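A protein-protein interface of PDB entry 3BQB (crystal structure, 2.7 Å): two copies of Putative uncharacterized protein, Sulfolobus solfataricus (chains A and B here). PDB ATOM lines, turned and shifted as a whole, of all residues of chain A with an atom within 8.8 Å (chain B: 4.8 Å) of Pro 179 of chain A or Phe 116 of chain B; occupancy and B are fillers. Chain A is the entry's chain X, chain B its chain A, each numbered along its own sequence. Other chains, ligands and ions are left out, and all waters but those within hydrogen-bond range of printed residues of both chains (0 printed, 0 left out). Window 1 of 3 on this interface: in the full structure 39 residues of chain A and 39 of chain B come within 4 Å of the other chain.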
ATOM      1  N   GLU A 114      31.669  -2.881 -21.077  1.00  0.00           N
ATOM      2  CA  GLU A 114      30.461  -2.518 -21.812  1.00  0.00           C
ATOM      3  C   GLU A 114      30.837  -1.997 -23.199  1.00  0.00           C
ATOM      4  O   GLU A 114      31.654  -1.081 -23.321  1.00  0.00           O
ATOM      5  CB  GLU A 114      29.688  -1.437 -21.054  1.00  0.00           C
ATOM      6  CG  GLU A 114      28.355  -1.020 -21.688  1.00  0.00           C
ATOM      7  CD  GLU A 114      27.694   0.144 -20.961  1.00  0.00           C
ATOM      8  OE1 GLU A 114      28.370   0.797 -20.138  1.00  0.00           O
ATOM      9  OE2 GLU A 114      26.500   0.412 -21.211  1.00  0.00           O
ATOM     10  N   PHE A 116      28.582  -0.968 -26.766  1.00  0.00           N
ATOM     11  CA  PHE A 116      27.243  -0.818 -27.331  1.00  0.00           C
ATOM     12  C   PHE A 116      27.269  -0.082 -28.669  1.00  0.00           C
ATOM     13  O   PHE A 116      28.144   0.746 -28.917  1.00  0.00           O
ATOM     14  CB  PHE A 116      26.317  -0.093 -26.344  1.00  0.00           C
ATOM     15  CG  PHE A 116      26.758   1.306 -25.994  1.00  0.00           C
ATOM     16  CD1 PHE A 116      26.272   2.402 -26.700  1.00  0.00           C
ATOM     17  CD2 PHE A 116      27.643   1.531 -24.946  1.00  0.00           C
ATOM     18  CE1 PHE A 116      26.670   3.698 -26.374  1.00  0.00           C
ATOM     19  CE2 PHE A 116      28.046   2.816 -24.616  1.00  0.00           C
ATOM     20  CZ  PHE A 116      27.557   3.902 -25.331  1.00  0.00           C
ATOM     21  N   PHE A 117      26.302  -0.393 -29.526  1.00  0.00           N
ATOM     22  CA  PHE A 117      26.163   0.286 -30.806  1.00  0.00           C
ATOM     23  C   PHE A 117      25.482   1.639 -30.586  1.00  0.00           C
ATOM     24  O   PHE A 117      24.435   1.716 -29.950  1.00  0.00           O
ATOM     25  CB  PHE A 117      25.361  -0.573 -31.790  1.00  0.00           C
ATOM     26  CG  PHE A 117      25.297   0.001 -33.172  1.00  0.00           C
ATOM     27  CD1 PHE A 117      24.217   0.766 -33.570  1.00  0.00           C
ATOM     28  CD2 PHE A 117      26.329  -0.207 -34.066  1.00  0.00           C
ATOM     29  CE1 PHE A 117      24.163   1.310 -34.844  1.00  0.00           C
ATOM     30  CE2 PHE A 117      26.283   0.329 -35.341  1.00  0.00           C
ATOM     31  CZ  PHE A 117      25.199   1.091 -35.730  1.00  0.00           C
ATOM     32  N   LYS A 118      26.081   2.698 -31.123  1.00  0.00           N
ATOM     33  CA  LYS A 118      25.627   4.067 -30.876  1.00  0.00           C
ATOM     34  C   LYS A 118      24.938   4.699 -32.090  1.00  0.00           C
ATOM     35  O   LYS A 118      23.885   5.315 -31.939  1.00  0.00           O
ATOM     36  CB  LYS A 118      26.812   4.930 -30.409  1.00  0.00           C
ATOM     37  CG  LYS A 118      26.536   6.425 -30.265  1.00  0.00           C
ATOM     38  CD  LYS A 118      25.435   6.728 -29.268  1.00  0.00           C
ATOM     39  CE  LYS A 118      25.102   8.204 -29.287  1.00  0.00           C
ATOM     40  NZ  LYS A 118      24.148   8.586 -28.220  1.00  0.00           N
ATOM     41  N   ALA A 119      25.514   4.565 -33.285  1.00  0.00           N
ATOM     42  CA  ALA A 119      24.962   5.270 -34.443  1.00  0.00           C
ATOM     43  C   ALA A 119      25.445   4.810 -35.813  1.00  0.00           C
ATOM     44  O   ALA A 119      26.456   4.121 -35.955  1.00  0.00           O
ATOM     45  CB  ALA A 119      25.226   6.770 -34.301  1.00  0.00           C
ATOM     46  N   ARG A 123      22.713   9.364 -38.482  1.00  0.00           N
ATOM     47  CA  ARG A 123      22.287   9.747 -37.131  1.00  0.00           C
ATOM     48  C   ARG A 123      23.284  10.679 -36.443  1.00  0.00           C
ATOM     49  O   ARG A 123      23.030  11.133 -35.328  1.00  0.00           O
ATOM     50  CB  ARG A 123      22.080   8.507 -36.259  1.00  0.00           C
ATOM     51  CG  ARG A 123      20.874   7.689 -36.655  1.00  0.00           C
ATOM     52  CD  ARG A 123      20.590   6.567 -35.659  1.00  0.00           C
ATOM     53  NE  ARG A 123      19.342   5.888 -36.010  1.00  0.00           N
ATOM     54  CZ  ARG A 123      19.237   4.906 -36.902  1.00  0.00           C
ATOM     55  NH1 ARG A 123      20.304   4.465 -37.554  1.00  0.00           N
ATOM     56  NH2 ARG A 123      18.048   4.368 -37.152  1.00  0.00           N
ATOM     57  N   ARG A 134      15.250  13.572 -27.461  1.00  0.00           N
ATOM     58  CA  ARG A 134      14.078  12.812 -27.896  1.00  0.00           C
ATOM     59  C   ARG A 134      12.805  13.473 -27.386  1.00  0.00           C
ATOM     60  O   ARG A 134      12.803  14.099 -26.329  1.00  0.00           O
ATOM     61  CB  ARG A 134      14.133  11.373 -27.387  1.00  0.00           C
ATOM     62  CG  ARG A 134      15.266  10.529 -27.957  1.00  0.00           C
ATOM     63  CD  ARG A 134      15.388   9.211 -27.196  1.00  0.00           C
ATOM     64  NE  ARG A 134      14.114   8.496 -27.196  1.00  0.00           N
ATOM     65  CZ  ARG A 134      13.723   7.608 -28.111  1.00  0.00           C
ATOM     66  NH1 ARG A 134      14.510   7.254 -29.125  1.00  0.00           N
ATOM     67  NH2 ARG A 134      12.521   7.056 -28.003  1.00  0.00           N
ATOM     68  N   VAL A 165      25.091  11.690 -26.783  1.00  0.00           N
ATOM     69  CA  VAL A 165      23.873  12.269 -26.210  1.00  0.00           C
ATOM     70  C   VAL A 165      22.976  11.140 -25.700  1.00  0.00           C
ATOM     71  O   VAL A 165      22.601  10.249 -26.466  1.00  0.00           O
ATOM     72  CB  VAL A 165      23.095  13.137 -27.237  1.00  0.00           C
ATOM     73  CG1 VAL A 165      21.940  13.873 -26.560  1.00  0.00           C
ATOM     74  CG2 VAL A 165      24.018  14.139 -27.927  1.00  0.00           C
ATOM     75  N   ALA A 167      19.580   9.861 -23.411  1.00  0.00           N
ATOM     76  CA  ALA A 167      18.314  10.010 -22.682  1.00  0.00           C
ATOM     77  C   ALA A 167      18.368   9.140 -21.422  1.00  0.00           C
ATOM     78  O   ALA A 167      17.871   8.015 -21.400  1.00  0.00           O
ATOM     79  CB  ALA A 167      17.137   9.629 -23.553  1.00  0.00           C
ATOM     80  N   LEU A 170      15.328   7.223 -19.671  1.00  0.00           N
ATOM     81  CA  LEU A 170      14.959   5.943 -20.283  1.00  0.00           C
ATOM     82  C   LEU A 170      15.889   4.805 -19.842  1.00  0.00           C
ATOM     83  O   LEU A 170      15.432   3.699 -19.570  1.00  0.00           O
ATOM     84  CB  LEU A 170      14.953   6.048 -21.809  1.00  0.00           C
ATOM     85  CG  LEU A 170      14.066   7.126 -22.444  1.00  0.00           C
ATOM     86  CD1 LEU A 170      14.123   6.983 -23.955  1.00  0.00           C
ATOM     87  CD2 LEU A 170      12.620   7.062 -21.956  1.00  0.00           C
ATOM     88  N   GLU A 171      17.188   5.083 -19.761  1.00  0.00           N
ATOM     89  CA  GLU A 171      18.157   4.101 -19.255  1.00  0.00           C
ATOM     90  C   GLU A 171      17.910   3.763 -17.783  1.00  0.00           C
ATOM     91  O   GLU A 171      18.151   2.635 -17.351  1.00  0.00           O
ATOM     92  CB  GLU A 171      19.583   4.618 -19.424  1.00  0.00           C
ATOM     93  CG  GLU A 171      20.660   3.633 -18.987  1.00  0.00           C
ATOM     94  CD  GLU A 171      22.059   4.220 -19.054  1.00  0.00           C
ATOM     95  OE1 GLU A 171      22.187   5.417 -19.390  1.00  0.00           O
ATOM     96  OE2 GLU A 171      23.032   3.485 -18.767  1.00  0.00           O
ATOM     97  N   ASN A 174      14.800   1.296 -17.296  1.00  0.00           N
ATOM     98  CA  ASN A 174      15.168  -0.081 -17.621  1.00  0.00           C
ATOM     99  C   ASN A 174      16.445  -0.104 -18.465  1.00  0.00           C
ATOM    100  O   ASN A 174      16.524   0.601 -19.473  1.00  0.00           O
ATOM    101  CB  ASN A 174      14.029  -0.765 -18.388  1.00  0.00           C
ATOM    102  CG  ASN A 174      14.014  -2.269 -18.194  1.00  0.00           C
ATOM    103  OD1 ASN A 174      15.044  -2.931 -18.300  1.00  0.00           O
ATOM    104  ND2 ASN A 174      12.839  -2.815 -17.899  1.00  0.00           N
ATOM    105  N   PRO A 175      17.449  -0.906 -18.062  1.00  0.00           N
ATOM    106  CA  PRO A 175      18.624  -1.012 -18.935  1.00  0.00           C
ATOM    107  C   PRO A 175      18.313  -1.536 -20.347  1.00  0.00           C
ATOM    108  O   PRO A 175      19.107  -1.317 -21.260  1.00  0.00           O
ATOM    109  CB  PRO A 175      19.559  -1.970 -18.180  1.00  0.00           C
ATOM    110  CG  PRO A 175      18.712  -2.646 -17.167  1.00  0.00           C
ATOM    111  CD  PRO A 175      17.600  -1.703 -16.833  1.00  0.00           C
ATOM    112  N   LEU A 176      17.171  -2.198 -20.530  1.00  0.00           N
ATOM    113  CA  LEU A 176      16.776  -2.690 -21.854  1.00  0.00           C
ATOM    114  C   LEU A 176      16.291  -1.574 -22.781  1.00  0.00           C
ATOM    115  O   LEU A 176      16.116  -1.801 -23.979  1.00  0.00           O
ATOM    116  CB  LEU A 176      15.708  -3.780 -21.735  1.00  0.00           C
ATOM    117  CG  LEU A 176      16.083  -4.985 -20.860  1.00  0.00           C
ATOM    118  CD1 LEU A 176      14.916  -5.974 -20.757  1.00  0.00           C
ATOM    119  CD2 LEU A 176      17.354  -5.667 -21.374  1.00  0.00           C
ATOM    120  N   TYR A 177      16.076  -0.376 -22.235  1.00  0.00           N
ATOM    121  CA  TYR A 177      15.800   0.810 -23.055  1.00  0.00           C
ATOM    122  C   TYR A 177      17.079   1.541 -23.507  1.00  0.00           C
ATOM    123  O   TYR A 177      17.002   2.541 -24.230  1.00  0.00           O
ATOM    124  CB  TYR A 177      14.890   1.791 -22.307  1.00  0.00           C
ATOM    125  CG  TYR A 177      13.569   1.215 -21.836  1.00  0.00           C
ATOM    126  CD1 TYR A 177      12.861   0.294 -22.611  1.00  0.00           C
ATOM    127  CD2 TYR A 177      13.009   1.612 -20.618  1.00  0.00           C
ATOM    128  CE1 TYR A 177      11.645  -0.229 -22.174  1.00  0.00           C
ATOM    129  CE2 TYR A 177      11.793   1.092 -20.174  1.00  0.00           C
ATOM    130  CZ  TYR A 177      11.117   0.175 -20.956  1.00  0.00           C
ATOM    131  OH  TYR A 177       9.916  -0.341 -20.523  1.00  0.00           O
ATOM    132  N   LEU A 178      18.247   1.035 -23.103  1.00  0.00           N
ATOM    133  CA  LEU A 178      19.531   1.644 -23.465  1.00  0.00           C
ATOM    134  C   LEU A 178      19.632   1.992 -24.959  1.00  0.00           C
ATOM    135  O   LEU A 178      20.007   3.118 -25.300  1.00  0.00           O
ATOM    136  CB  LEU A 178      20.696   0.738 -23.039  1.00  0.00           C
ATOM    137  CG  LEU A 178      22.115   1.293 -23.128  1.00  0.00           C
ATOM    138  CD1 LEU A 178      22.324   2.400 -22.097  1.00  0.00           C
ATOM    139  CD2 LEU A 178      23.133   0.168 -22.927  1.00  0.00           C
ATOM    140  N   PRO A 179      19.295   1.039 -25.853  1.00  0.00           N
ATOM    141  CA  PRO A 179      19.352   1.347 -27.282  1.00  0.00           C
ATOM    142  C   PRO A 179      18.458   2.512 -27.706  1.00  0.00           C
ATOM    143  O   PRO A 179      18.867   3.324 -28.534  1.00  0.00           O
ATOM    144  CB  PRO A 179      18.881   0.044 -27.935  1.00  0.00           C
ATOM    145  CG  PRO A 179      19.156  -1.000 -26.934  1.00  0.00           C
ATOM    146  CD  PRO A 179      18.868  -0.353 -25.631  1.00  0.00           C
ATOM    147  N   GLN A 180      17.255   2.595 -27.145  1.00  0.00           N
ATOM    148  CA  GLN A 180      16.357   3.719 -27.427  1.00  0.00           C
ATOM    149  C   GLN A 180      16.908   5.043 -26.883  1.00  0.00           C
ATOM    150  O   GLN A 180      16.666   6.096 -27.466  1.00  0.00           O
ATOM    151  CB  GLN A 180      14.963   3.463 -26.848  1.00  0.00           C
ATOM    152  CG  GLN A 180      14.208   2.325 -27.511  1.00  0.00           C
ATOM    153  CD  GLN A 180      12.924   1.969 -26.785  1.00  0.00           C
ATOM    154  OE1 GLN A 180      11.934   2.707 -26.849  1.00  0.00           O
ATOM    155  NE2 GLN A 180      12.929   0.829 -26.096  1.00  0.00           N
ATOM    156  N   SER A 181      17.640   4.980 -25.769  1.00  0.00           N
ATOM    157  CA  SER A 181      18.242   6.173 -25.165  1.00  0.00           C
ATOM    158  C   SER A 181      19.469   6.685 -25.932  1.00  0.00           C
ATOM    159  O   SER A 181      19.731   7.888 -25.940  1.00  0.00           O
ATOM    160  CB  SER A 181      18.622   5.914 -23.703  1.00  0.00           C
ATOM    161  OG  SER A 181      19.703   5.009 -23.591  1.00  0.00           O
ATOM    162  N   LYS A 182      20.206   5.774 -26.570  1.00  0.00           N
ATOM    163  CA  LYS A 182      21.456   6.115 -27.253  1.00  0.00           C
ATOM    164  C   LYS A 182      21.304   6.347 -28.761  1.00  0.00           C
ATOM    165  O   LYS A 182      22.085   7.097 -29.345  1.00  0.00           O
ATOM    166  CB  LYS A 182      22.491   5.011 -27.032  1.00  0.00           C
ATOM    167  CG  LYS A 182      22.938   4.833 -25.580  1.00  0.00           C
ATOM    168  CD  LYS A 182      23.888   5.939 -25.130  1.00  0.00           C
ATOM    169  CE  LYS A 182      24.530   5.615 -23.784  1.00  0.00           C
ATOM    170  NZ  LYS A 182      25.401   6.722 -23.299  1.00  0.00           N
ATOM    171  N   ILE A 183      20.311   5.710 -29.387  1.00  0.00           N
ATOM    172  CA  ILE A 183      20.251   5.633 -30.851  1.00  0.00           C
ATOM    173  C   ILE A 183      19.007   6.324 -31.433  1.00  0.00           C
ATOM    174  O   ILE A 183      17.895   5.786 -31.370  1.00  0.00           O
ATOM    175  CB  ILE A 183      20.315   4.157 -31.336  1.00  0.00           C
ATOM    176  CG1 ILE A 183      21.384   3.379 -30.555  1.00  0.00           C
ATOM    177  CG2 ILE A 183      20.614   4.096 -32.837  1.00  0.00           C
ATOM    178  CD1 ILE A 183      21.366   1.878 -30.791  1.00  0.00           C
ATOM    179  N   TYR A 184      19.210   7.512 -32.004  1.00  0.00           N
ATOM    180  CA  TYR A 184      18.138   8.278 -32.649  1.00  0.00           C
ATOM    181  C   TYR A 184      18.715   9.418 -33.499  1.00  0.00           C
ATOM    182  O   TYR A 184      19.921   9.668 -33.472  1.00  0.00           O
ATOM    183  CB  TYR A 184      17.146   8.822 -31.605  1.00  0.00           C
ATOM    184  CG  TYR A 184      17.777   9.690 -30.535  1.00  0.00           C
ATOM    185  CD1 TYR A 184      17.814  11.075 -30.669  1.00  0.00           C
ATOM    186  CD2 TYR A 184      18.337   9.128 -29.394  1.00  0.00           C
ATOM    187  CE1 TYR A 184      18.391  11.878 -29.691  1.00  0.00           C
ATOM    188  CE2 TYR A 184      18.922   9.921 -28.416  1.00  0.00           C
ATOM    189  CZ  TYR A 184      18.945  11.294 -28.568  1.00  0.00           C
ATOM    190  OH  TYR A 184      19.528  12.075 -27.592  1.00  0.00           O
ATOM    191  N   CYS A 187      21.543  11.963 -32.212  1.00  0.00           N
ATOM    192  CA  CYS A 187      21.944  11.421 -30.904  1.00  0.00           C
ATOM    193  C   CYS A 187      23.460  11.421 -30.673  1.00  0.00           C
ATOM    194  O   CYS A 187      23.931  10.983 -29.615  1.00  0.00           O
ATOM    195  CB  CYS A 187      21.455   9.978 -30.775  1.00  0.00           C
ATOM    196  SG  CYS A 187      22.315   8.830 -31.894  1.00  0.00           S
ATOM    197  N   VAL B  76      18.854  -3.779 -39.217  1.00  0.00           N
ATOM    198  CA  VAL B  76      17.980  -4.771 -38.610  1.00  0.00           C
ATOM    199  C   VAL B  76      17.822  -4.454 -37.133  1.00  0.00           C
ATOM    200  O   VAL B  76      18.809  -4.348 -36.412  1.00  0.00           O
ATOM    201  CB  VAL B  76      18.531  -6.201 -38.752  1.00  0.00           C
ATOM    202  CG1 VAL B  76      17.530  -7.209 -38.183  1.00  0.00           C
ATOM    203  CG2 VAL B  76      18.847  -6.515 -40.211  1.00  0.00           C
ATOM    204  N   TRP B  77      16.580  -4.303 -36.691  1.00  0.00           N
ATOM    205  CA  TRP B  77      16.281  -4.069 -35.282  1.00  0.00           C
ATOM    206  C   TRP B  77      15.494  -5.242 -34.706  1.00  0.00           C
ATOM    207  O   TRP B  77      14.865  -6.002 -35.437  1.00  0.00           O
ATOM    208  CB  TRP B  77      15.485  -2.773 -35.117  1.00  0.00           C
ATOM    209  CG  TRP B  77      16.266  -1.524 -35.453  1.00  0.00           C
ATOM    210  CD1 TRP B  77      16.618  -1.086 -36.700  1.00  0.00           C
ATOM    211  CD2 TRP B  77      16.768  -0.548 -34.531  1.00  0.00           C
ATOM    212  NE1 TRP B  77      17.312   0.092 -36.609  1.00  0.00           N
ATOM    213  CE2 TRP B  77      17.417   0.448 -35.291  1.00  0.00           C
ATOM    214  CE3 TRP B  77      16.731  -0.419 -33.139  1.00  0.00           C
ATOM    215  CZ2 TRP B  77      18.031   1.558 -34.704  1.00  0.00           C
ATOM    216  CZ3 TRP B  77      17.340   0.682 -32.556  1.00  0.00           C
ATOM    217  CH2 TRP B  77      17.980   1.657 -33.338  1.00  0.00           C
ATOM    218  N   GLY B  78      15.540  -5.380 -33.387  1.00  0.00           N
ATOM    219  CA  GLY B  78      14.826  -6.442 -32.689  1.00  0.00           C
ATOM    220  C   GLY B  78      13.899  -5.890 -31.627  1.00  0.00           C
ATOM    221  O   GLY B  78      13.904  -4.690 -31.347  1.00  0.00           O
ATOM    222  N   SER B  79      13.092  -6.772 -31.044  1.00  0.00           N
ATOM    223  CA  SER B  79      12.181  -6.402 -29.967  1.00  0.00           C
ATOM    224  C   SER B  79      11.939  -7.596 -29.056  1.00  0.00           C
ATOM    225  O   SER B  79      11.261  -8.543 -29.440  1.00  0.00           O
ATOM    226  CB  SER B  79      10.856  -5.905 -30.543  1.00  0.00           C
ATOM    227  OG  SER B  79      10.018  -5.412 -29.515  1.00  0.00           O
ATOM    228  N   GLY B  80      12.497  -7.558 -27.851  1.00  0.00           N
ATOM    229  CA  GLY B  80      12.428  -8.704 -26.946  1.00  0.00           C
ATOM    230  C   GLY B  80      11.165  -8.759 -26.103  1.00  0.00           C
ATOM    231  O   GLY B  80      10.499  -7.745 -25.899  1.00  0.00           O
ATOM    232  N   GLU B 114      10.878  -3.379 -25.345  1.00  0.00           N
ATOM    233  CA  GLU B 114      12.297  -3.452 -25.681  1.00  0.00           C
ATOM    234  C   GLU B 114      12.457  -3.309 -27.196  1.00  0.00           C
ATOM    235  O   GLU B 114      11.821  -4.027 -27.973  1.00  0.00           O
ATOM    236  CB  GLU B 114      12.935  -4.760 -25.197  1.00  0.00           C
ATOM    237  CG  GLU B 114      14.443  -4.849 -25.474  1.00  0.00           C
ATOM    238  CD  GLU B 114      15.098  -6.108 -24.914  1.00  0.00           C
ATOM    239  OE1 GLU B 114      14.383  -7.076 -24.583  1.00  0.00           O
ATOM    240  OE2 GLU B 114      16.340  -6.131 -24.808  1.00  0.00           O
ATOM    241  N   ILE B 115      13.280  -2.343 -27.592  1.00  0.00           N
ATOM    242  CA  ILE B 115      13.693  -2.147 -28.973  1.00  0.00           C
ATOM    243  C   ILE B 115      15.209  -2.079 -28.941  1.00  0.00           C
ATOM    244  O   ILE B 115      15.766  -1.318 -28.150  1.00  0.00           O
ATOM    245  CB  ILE B 115      13.163  -0.817 -29.545  1.00  0.00           C
ATOM    246  CG1 ILE B 115      11.631  -0.809 -29.583  1.00  0.00           C
ATOM    247  CG2 ILE B 115      13.730  -0.558 -30.943  1.00  0.00           C
ATOM    248  CD1 ILE B 115      11.022  -1.662 -30.680  1.00  0.00           C
ATOM    249  N   PHE B 116      15.874  -2.879 -29.772  1.00  0.00           N
ATOM    250  CA  PHE B 116      17.337  -2.861 -29.850  1.00  0.00           C
ATOM    251  C   PHE B 116      17.844  -3.039 -31.283  1.00  0.00           C
ATOM    252  O   PHE B 116      17.159  -3.618 -32.126  1.00  0.00           O
ATOM    253  CB  PHE B 116      17.939  -3.929 -28.932  1.00  0.00           C
ATOM    254  CG  PHE B 116      17.564  -5.333 -29.303  1.00  0.00           C
ATOM    255  CD1 PHE B 116      18.403  -6.106 -30.095  1.00  0.00           C
ATOM    256  CD2 PHE B 116      16.373  -5.888 -28.857  1.00  0.00           C
ATOM    257  CE1 PHE B 116      18.056  -7.410 -30.434  1.00  0.00           C
ATOM    258  CE2 PHE B 116      16.021  -7.188 -29.193  1.00  0.00           C
ATOM    259  CZ  PHE B 116      16.864  -7.949 -29.979  1.00  0.00           C
ATOM    260  N   PHE B 117      19.043  -2.517 -31.544  1.00  0.00           N
ATOM    261  CA  PHE B 117      19.690  -2.641 -32.847  1.00  0.00           C
ATOM    262  C   PHE B 117      20.307  -4.038 -32.940  1.00  0.00           C
ATOM    263  O   PHE B 117      21.013  -4.460 -32.032  1.00  0.00           O
ATOM    264  CB  PHE B 117      20.756  -1.548 -33.016  1.00  0.00           C
ATOM    265  CG  PHE B 117      21.393  -1.520 -34.379  1.00  0.00           C
ATOM    266  CD1 PHE B 117      22.649  -2.073 -34.587  1.00  0.00           C
ATOM    267  CD2 PHE B 117      20.735  -0.944 -35.456  1.00  0.00           C
ATOM    268  CE1 PHE B 117      23.236  -2.052 -35.843  1.00  0.00           C
ATOM    269  CE2 PHE B 117      21.319  -0.919 -36.718  1.00  0.00           C
ATOM    270  CZ  PHE B 117      22.571  -1.475 -36.909  1.00  0.00           C
ATOM    271  N   LYS B 118      20.034  -4.748 -34.034  1.00  0.00           N
ATOM    272  CA  LYS B 118      20.455  -6.145 -34.174  1.00  0.00           C
ATOM    273  C   LYS B 118      21.593  -6.331 -35.181  1.00  0.00           C
ATOM    274  O   LYS B 118      22.597  -6.966 -34.864  1.00  0.00           O
ATOM    275  CB  LYS B 118      19.252  -7.035 -34.539  1.00  0.00           C
ATOM    276  CG  LYS B 118      19.591  -8.498 -34.847  1.00  0.00           C
ATOM    277  CD  LYS B 118      20.325  -9.188 -33.702  1.00  0.00           C
ATOM    278  CE  LYS B 118      20.820 -10.570 -34.108  1.00  0.00           C
ATOM    279  NZ  LYS B 118      21.492 -11.299 -32.980  1.00  0.00           N
ATOM    280  N   ASP B 164      17.335 -14.563 -34.610  1.00  0.00           N
ATOM    281  CA  ASP B 164      18.106 -13.638 -33.779  1.00  0.00           C
ATOM    282  C   ASP B 164      19.066 -14.457 -32.923  1.00  0.00           C
ATOM    283  O   ASP B 164      18.755 -14.799 -31.789  1.00  0.00           O
ATOM    284  CB  ASP B 164      17.160 -12.784 -32.916  1.00  0.00           C
ATOM    285  CG  ASP B 164      17.897 -11.818 -31.979  1.00  0.00           C
ATOM    286  OD1 ASP B 164      19.140 -11.874 -31.861  1.00  0.00           O
ATOM    287  OD2 ASP B 164      17.210 -10.999 -31.338  1.00  0.00           O
ATOM    288  N   LYS B 182      24.233  -9.839 -29.180  1.00  0.00           N
ATOM    289  CA  LYS B 182      23.324  -9.765 -30.323  1.00  0.00           C
ATOM    290  C   LYS B 182      24.004  -9.408 -31.657  1.00  0.00           C
ATOM    291  O   LYS B 182      23.517  -9.795 -32.715  1.00  0.00           O
ATOM    292  CB  LYS B 182      22.224  -8.733 -30.035  1.00  0.00           C
ATOM    293  CG  LYS B 182      21.289  -9.094 -28.883  1.00  0.00           C
ATOM    294  CD  LYS B 182      20.338 -10.220 -29.265  1.00  0.00           C
ATOM    295  CE  LYS B 182      19.272 -10.451 -28.211  1.00  0.00           C
ATOM    296  NZ  LYS B 182      18.258 -11.431 -28.696  1.00  0.00           N
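N of Gly 78 of chain B lies within hydrogen-bond range of O of Phe 116 of chain B, at 2.7 Å.
The side-chain hydroxyl (OG) of Ser 79 of chain B is in hydrogen-bond range of the backbone carbonyl oxygen (O) of Glu 114 of chain B, 2.7 Å away.
The backbone carbonyl oxygen (O) of Gln 180 of chain A is in hydrogen-bond range of the guanidinium group (NH1) of Arg 134 of chain A, at 3.0 Å.
OD1 of Asn 174 of chain A lies close to N of Leu 176 of chain A (3.2 Å).
Among the printed residues, pairs that only touch across the chains: Phe 117 of chain A with Phe 117 of chain B, Pro 179 of chain A with Ile 115 of chain B, Gln 180 of chain A with Ile 115 of chain B, Leu 176 of chain A with Glu 114 of chain B, Ile 183 of chain A with Trp 77 of chain B, Arg 123 of chain A with Trp 77 of chain B and Pro 179 of chain A with Phe 116 of chain B.
Of chain B, only Ile 115 and Phe 116 come within 4 Å of Pro 179 of chain A.
Phe 116 of chain B touches one residue of chain A.
No residue of chain A comes within 4 Å of Gly 78 of chain B.
Of the printed residues of chain B, Ile 183 of chain A touches Trp 77.
Of the printed residues of chain B, Phe 117 of chain A touches Phe 117 (3.4 Å).
Asp 164 of chain B touches none of the printed residues of chain A.
Pro 175 of chain A touches none of the printed residues of chain B.
The nearest residue of chain A that does not touch Phe 116 of chain B is Leu 176 of chain A (5.7 Å).
Printed residues of chain B that touch a printed residue of chain A: Trp 77, Glu 114, Ile 115, Phe 116 and Phe 117.
Hydrophobic or aromatic side chains of chain B within 4 Å of the printed part of chain A: Trp 77, Ile 115, Phe 116 and Phe 117.
Hydrophobic or aromatic side chains of chain A that line the printed part of chain B: Phe 117, Leu 176, Pro 179 and Ile 183.
Phe 117 of chain B touches its own counterpart, Phe 117 of chain A.
5 positions are printed for both chains.
Of the 7 pairs that touch across the chains among the printed residues, 1 has its exchanged pair printed and touching as well.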
